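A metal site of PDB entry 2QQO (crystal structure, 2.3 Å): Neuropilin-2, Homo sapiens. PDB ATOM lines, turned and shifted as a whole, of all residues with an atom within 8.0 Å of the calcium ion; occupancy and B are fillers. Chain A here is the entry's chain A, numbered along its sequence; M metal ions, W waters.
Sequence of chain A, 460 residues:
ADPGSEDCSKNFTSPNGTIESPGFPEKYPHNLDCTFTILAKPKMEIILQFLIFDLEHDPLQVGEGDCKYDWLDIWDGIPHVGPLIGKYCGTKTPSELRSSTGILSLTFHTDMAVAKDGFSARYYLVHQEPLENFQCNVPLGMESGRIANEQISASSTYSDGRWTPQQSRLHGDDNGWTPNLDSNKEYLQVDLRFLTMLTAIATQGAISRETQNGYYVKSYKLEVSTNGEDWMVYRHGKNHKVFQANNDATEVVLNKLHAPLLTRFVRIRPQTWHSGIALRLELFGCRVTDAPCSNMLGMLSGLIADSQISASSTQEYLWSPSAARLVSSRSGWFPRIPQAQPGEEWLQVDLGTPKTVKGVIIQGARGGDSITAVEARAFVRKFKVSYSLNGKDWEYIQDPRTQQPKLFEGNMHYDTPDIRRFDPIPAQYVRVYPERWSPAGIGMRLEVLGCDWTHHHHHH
Within 4 Å of the calcium ion: Glu 56, Asp 70, Asp 111, Ala 113 and Val 114.
The nearest printed residue that does not touch the calcium ion is His 30 (4.6 Å).
Water W1 bridges O of Asp 111 (2.6 Å) and ND1 of His 30 (2.7 Å).
The calcium ion is bound by OD1 of Asp 111 (2.3 Å), water W1 (2.3 Å), O of Ala 113 (2.4 Å), O of Val 114 (2.4 Å), OE1 of Glu 56 (2.6 Å), OD2 of Asp 70 (2.6 Å) and OD1 of Asp 70 (2.7 Å).
The calcium ion has seven donor atoms within binding distance.
O of Asp 111 lies within hydrogen-bond range of N of Asn 31 (3.1 Å).
The side-chain hydroxyl (OH) of Tyr 28 lies within hydrogen-bond range of the backbone NH (N) of Glu 56 (3.1 Å).
The side-chain carboxylate (OD2) of Asp 70 lies close to the side-chain hydroxyl (OH) of Tyr 28.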
ATOM      1  N   TYR A  28     -15.666 -23.879  20.474  1.00  0.00           N
ATOM      2  CA  TYR A  28     -16.151 -23.200  21.680  1.00  0.00           C
ATOM      3  C   TYR A  28     -16.261 -24.173  22.869  1.00  0.00           C
ATOM      4  O   TYR A  28     -16.520 -25.361  22.678  1.00  0.00           O
ATOM      5  CB  TYR A  28     -17.479 -22.446  21.418  1.00  0.00           C
ATOM      6  CG  TYR A  28     -18.686 -23.248  20.903  1.00  0.00           C
ATOM      7  CD1 TYR A  28     -19.186 -23.027  19.618  1.00  0.00           C
ATOM      8  CD2 TYR A  28     -19.341 -24.197  21.698  1.00  0.00           C
ATOM      9  CE1 TYR A  28     -20.302 -23.725  19.126  1.00  0.00           C
ATOM     10  CE2 TYR A  28     -20.458 -24.921  21.228  1.00  0.00           C
ATOM     11  CZ  TYR A  28     -20.933 -24.673  19.938  1.00  0.00           C
ATOM     12  OH  TYR A  28     -22.009 -25.357  19.427  1.00  0.00           O
ATOM     13  N   PRO A  29     -16.019 -23.667  24.094  1.00  0.00           N
ATOM     14  CA  PRO A  29     -16.167 -24.460  25.323  1.00  0.00           C
ATOM     15  C   PRO A  29     -17.591 -24.908  25.610  1.00  0.00           C
ATOM     16  O   PRO A  29     -18.554 -24.325  25.110  1.00  0.00           O
ATOM     17  CB  PRO A  29     -15.724 -23.490  26.435  1.00  0.00           C
ATOM     18  CG  PRO A  29     -14.935 -22.459  25.764  1.00  0.00           C
ATOM     19  CD  PRO A  29     -15.524 -22.309  24.402  1.00  0.00           C
ATOM     20  N   HIS A  30     -17.701 -25.912  26.486  1.00  0.00           N
ATOM     21  CA  HIS A  30     -18.993 -26.382  26.980  1.00  0.00           C
ATOM     22  C   HIS A  30     -19.443 -25.601  28.223  1.00  0.00           C
ATOM     23  O   HIS A  30     -18.647 -24.961  28.899  1.00  0.00           O
ATOM     24  CB  HIS A  30     -18.898 -27.871  27.303  1.00  0.00           C
ATOM     25  CG  HIS A  30     -18.442 -28.699  26.151  1.00  0.00           C
ATOM     26  ND1 HIS A  30     -19.111 -28.725  24.936  1.00  0.00           N
ATOM     27  CD2 HIS A  30     -17.369 -29.521  26.002  1.00  0.00           C
ATOM     28  CE1 HIS A  30     -18.475 -29.526  24.104  1.00  0.00           C
ATOM     29  NE2 HIS A  30     -17.416 -30.012  24.717  1.00  0.00           N
ATOM     30  N   ASN A  31     -20.746 -25.668  28.500  1.00  0.00           N
ATOM     31  CA  ASN A  31     -21.353 -25.092  29.712  1.00  0.00           C
ATOM     32  C   ASN A  31     -21.197 -23.573  29.848  1.00  0.00           C
ATOM     33  O   ASN A  31     -21.028 -23.056  30.952  1.00  0.00           O
ATOM     34  CB  ASN A  31     -20.808 -25.801  30.959  1.00  0.00           C
ATOM     35  CG  ASN A  31     -20.865 -27.306  30.836  1.00  0.00           C
ATOM     36  OD1 ASN A  31     -21.940 -27.894  30.785  1.00  0.00           O
ATOM     37  ND2 ASN A  31     -19.693 -27.937  30.792  1.00  0.00           N
ATOM     38  N   LEU A  55     -22.856 -23.254  15.004  1.00  0.00           N
ATOM     39  CA  LEU A  55     -23.268 -23.807  16.308  1.00  0.00           C
ATOM     40  C   LEU A  55     -23.941 -25.176  16.098  1.00  0.00           C
ATOM     41  O   LEU A  55     -24.536 -25.433  15.039  1.00  0.00           O
ATOM     42  CB  LEU A  55     -24.267 -22.854  17.004  1.00  0.00           C
ATOM     43  CG  LEU A  55     -23.739 -21.731  17.916  1.00  0.00           C
ATOM     44  CD1 LEU A  55     -22.820 -20.786  17.177  1.00  0.00           C
ATOM     45  CD2 LEU A  55     -24.926 -20.975  18.557  1.00  0.00           C
ATOM     46  N   GLU A  56     -23.853 -26.040  17.094  1.00  0.00           N
ATOM     47  CA  GLU A  56     -24.643 -27.288  17.141  1.00  0.00           C
ATOM     48  C   GLU A  56     -26.146 -27.065  16.905  1.00  0.00           C
ATOM     49  O   GLU A  56     -26.735 -26.154  17.495  1.00  0.00           O
ATOM     50  CB  GLU A  56     -24.447 -27.948  18.511  1.00  0.00           C
ATOM     51  CG  GLU A  56     -25.070 -29.344  18.639  1.00  0.00           C
ATOM     52  CD  GLU A  56     -25.104 -29.828  20.069  1.00  0.00           C
ATOM     53  OE1 GLU A  56     -24.752 -29.063  21.003  1.00  0.00           O
ATOM     54  OE2 GLU A  56     -25.471 -31.007  20.262  1.00  0.00           O
ATOM     55  N   HIS A  57     -26.756 -27.925  16.069  1.00  0.00           N
ATOM     56  CA  HIS A  57     -28.201 -27.863  15.784  1.00  0.00           C
ATOM     57  C   HIS A  57     -28.965 -29.000  16.475  1.00  0.00           C
ATOM     58  O   HIS A  57     -28.421 -30.076  16.726  1.00  0.00           O
ATOM     59  CB  HIS A  57     -28.454 -27.887  14.258  1.00  0.00           C
ATOM     60  CG  HIS A  57     -28.931 -29.217  13.739  1.00  0.00           C
ATOM     61  ND1 HIS A  57     -28.076 -30.209  13.304  1.00  0.00           N
ATOM     62  CD2 HIS A  57     -30.184 -29.711  13.556  1.00  0.00           C
ATOM     63  CE1 HIS A  57     -28.778 -31.252  12.893  1.00  0.00           C
ATOM     64  NE2 HIS A  57     -30.059 -30.977  13.042  1.00  0.00           N
ATOM     65  N   TYR A  69     -30.154 -26.994  22.186  1.00  0.00           N
ATOM     66  CA  TYR A  69     -28.888 -27.407  22.783  1.00  0.00           C
ATOM     67  C   TYR A  69     -27.939 -26.239  22.950  1.00  0.00           C
ATOM     68  O   TYR A  69     -27.719 -25.800  24.069  1.00  0.00           O
ATOM     69  CB  TYR A  69     -28.220 -28.509  21.939  1.00  0.00           C
ATOM     70  CG  TYR A  69     -28.953 -29.851  21.914  1.00  0.00           C
ATOM     71  CD1 TYR A  69     -29.060 -30.582  20.734  1.00  0.00           C
ATOM     72  CD2 TYR A  69     -29.499 -30.400  23.083  1.00  0.00           C
ATOM     73  CE1 TYR A  69     -29.691 -31.817  20.715  1.00  0.00           C
ATOM     74  CE2 TYR A  69     -30.138 -31.630  23.064  1.00  0.00           C
ATOM     75  CZ  TYR A  69     -30.226 -32.345  21.884  1.00  0.00           C
ATOM     76  OH  TYR A  69     -30.870 -33.583  21.861  1.00  0.00           O
ATOM     77  N   ASP A  70     -27.358 -25.762  21.842  1.00  0.00           N
ATOM     78  CA  ASP A  70     -26.550 -24.529  21.824  1.00  0.00           C
ATOM     79  C   ASP A  70     -27.280 -23.451  21.005  1.00  0.00           C
ATOM     80  O   ASP A  70     -27.940 -23.758  20.023  1.00  0.00           O
ATOM     81  CB  ASP A  70     -25.177 -24.761  21.178  1.00  0.00           C
ATOM     82  CG  ASP A  70     -24.353 -25.779  21.919  1.00  0.00           C
ATOM     83  OD1 ASP A  70     -24.676 -26.116  23.066  1.00  0.00           O
ATOM     84  OD2 ASP A  70     -23.360 -26.246  21.334  1.00  0.00           O
ATOM     85  N   TRP A  71     -27.145 -22.189  21.405  1.00  0.00           N
ATOM     86  CA  TRP A  71     -27.800 -21.094  20.699  1.00  0.00           C
ATOM     87  C   TRP A  71     -27.202 -19.735  21.015  1.00  0.00           C
ATOM     88  O   TRP A  71     -26.560 -19.558  22.053  1.00  0.00           O
ATOM     89  CB  TRP A  71     -29.297 -21.045  21.036  1.00  0.00           C
ATOM     90  CG  TRP A  71     -29.611 -20.682  22.464  1.00  0.00           C
ATOM     91  CD1 TRP A  71     -29.569 -19.431  23.034  1.00  0.00           C
ATOM     92  CD2 TRP A  71     -30.003 -21.581  23.502  1.00  0.00           C
ATOM     93  NE1 TRP A  71     -29.914 -19.498  24.360  1.00  0.00           N
ATOM     94  CE2 TRP A  71     -30.203 -20.809  24.671  1.00  0.00           C
ATOM     95  CE3 TRP A  71     -30.208 -22.969  23.561  1.00  0.00           C
ATOM     96  CZ2 TRP A  71     -30.608 -21.378  25.889  1.00  0.00           C
ATOM     97  CZ3 TRP A  71     -30.613 -23.538  24.778  1.00  0.00           C
ATOM     98  CH2 TRP A  71     -30.808 -22.752  25.921  1.00  0.00           C
ATOM     99  N   HIS A 109     -25.274 -19.403  24.686  1.00  0.00           N
ATOM    100  CA  HIS A 109     -25.472 -20.533  25.574  1.00  0.00           C
ATOM    101  C   HIS A 109     -24.898 -21.810  24.953  1.00  0.00           C
ATOM    102  O   HIS A 109     -25.192 -22.102  23.793  1.00  0.00           O
ATOM    103  CB  HIS A 109     -26.965 -20.722  25.845  1.00  0.00           C
ATOM    104  CG  HIS A 109     -27.276 -21.945  26.652  1.00  0.00           C
ATOM    105  ND1 HIS A 109     -27.214 -21.958  28.035  1.00  0.00           N
ATOM    106  CD2 HIS A 109     -27.577 -23.202  26.272  1.00  0.00           C
ATOM    107  CE1 HIS A 109     -27.498 -23.173  28.464  1.00  0.00           C
ATOM    108  NE2 HIS A 109     -27.717 -23.944  27.413  1.00  0.00           N
ATOM    109  N   THR A 110     -24.099 -22.558  25.726  1.00  0.00           N
ATOM    110  CA  THR A 110     -23.666 -23.904  25.328  1.00  0.00           C
ATOM    111  C   THR A 110     -23.937 -24.951  26.427  1.00  0.00           C
ATOM    112  O   THR A 110     -23.861 -24.650  27.631  1.00  0.00           O
ATOM    113  CB  THR A 110     -22.168 -23.947  24.961  1.00  0.00           C
ATOM    114  OG1 THR A 110     -21.376 -23.656  26.118  1.00  0.00           O
ATOM    115  CG2 THR A 110     -21.845 -22.948  23.847  1.00  0.00           C
ATOM    116  N   ASP A 111     -24.275 -26.166  26.015  1.00  0.00           N
ATOM    117  CA  ASP A 111     -24.551 -27.261  26.963  1.00  0.00           C
ATOM    118  C   ASP A 111     -23.316 -28.182  27.179  1.00  0.00           C
ATOM    119  O   ASP A 111     -22.189 -27.844  26.758  1.00  0.00           O
ATOM    120  CB  ASP A 111     -25.809 -28.043  26.528  1.00  0.00           C
ATOM    121  CG  ASP A 111     -25.615 -28.803  25.217  1.00  0.00           C
ATOM    122  OD1 ASP A 111     -24.485 -28.874  24.712  1.00  0.00           O
ATOM    123  OD2 ASP A 111     -26.625 -29.339  24.703  1.00  0.00           O
ATOM    124  N   MET A 112     -23.549 -29.335  27.820  1.00  0.00           N
ATOM    125  CA  MET A 112     -22.457 -30.189  28.318  1.00  0.00           C
ATOM    126  C   MET A 112     -21.587 -30.895  27.258  1.00  0.00           C
ATOM    127  O   MET A 112     -20.440 -31.244  27.547  1.00  0.00           O
ATOM    128  CB  MET A 112     -22.988 -31.202  29.353  1.00  0.00           C
ATOM    129  CG  MET A 112     -23.757 -32.391  28.797  1.00  0.00           C
ATOM    130  SD  MET A 112     -25.375 -32.007  28.111  1.00  0.00           S
ATOM    131  CE  MET A 112     -26.382 -32.022  29.596  1.00  0.00           C
ATOM    132  N   ALA A 113     -22.117 -31.111  26.050  1.00  0.00           N
ATOM    133  CA  ALA A 113     -21.357 -31.809  24.997  1.00  0.00           C
ATOM    134  C   ALA A 113     -21.621 -31.268  23.565  1.00  0.00           C
ATOM    135  O   ALA A 113     -22.611 -30.609  23.327  1.00  0.00           O
ATOM    136  CB  ALA A 113     -21.664 -33.304  25.050  1.00  0.00           C
ATOM    137  N   VAL A 114     -20.708 -31.571  22.640  1.00  0.00           N
ATOM    138  CA  VAL A 114     -20.795 -31.170  21.225  1.00  0.00           C
ATOM    139  C   VAL A 114     -20.548 -29.672  20.992  1.00  0.00           C
ATOM    140  O   VAL A 114     -21.366 -28.815  21.376  1.00  0.00           O
ATOM    141  CB  VAL A 114     -22.114 -31.597  20.552  1.00  0.00           C
ATOM    142  CG1 VAL A 114     -22.008 -31.457  19.038  1.00  0.00           C
ATOM    143  CG2 VAL A 114     -22.467 -33.038  20.921  1.00  0.00           C
ATOM    144  N   ALA A 115     -19.422 -29.383  20.352  1.00  0.00           N
ATOM    145  CA  ALA A 115     -18.968 -28.031  20.115  1.00  0.00           C
ATOM    146  C   ALA A 115     -18.602 -27.858  18.642  1.00  0.00           C
ATOM    147  O   ALA A 115     -18.306 -28.834  17.966  1.00  0.00           O
ATOM    148  CB  ALA A 115     -17.791 -27.737  20.990  1.00  0.00           C
ATOM    149  N   LYS A 116     -18.665 -26.624  18.149  1.00  0.00           N
ATOM    150  CA  LYS A 116     -18.318 -26.326  16.747  1.00  0.00           C
ATOM    151  C   LYS A 116     -17.406 -25.088  16.728  1.00  0.00           C
ATOM    152  O   LYS A 116     -16.908 -24.712  17.773  1.00  0.00           O
ATOM    153  CB  LYS A 116     -19.588 -26.117  15.909  1.00  0.00           C
ATOM    154  CG  LYS A 116     -20.613 -27.272  15.963  1.00  0.00           C
ATOM    155  CD  LYS A 116     -20.137 -28.491  15.171  1.00  0.00           C
ATOM    156  CE  LYS A 116     -21.110 -29.650  15.312  1.00  0.00           C
ATOM    157  NZ  LYS A 116     -20.704 -30.848  14.508  1.00  0.00           N
HETATM  158 CA    CA M   1     -23.207 -28.334  22.908  1.00  0.00          CA
HETATM  159  O   HOH W   1     -21.436 -27.621  24.265  1.00  0.00           O
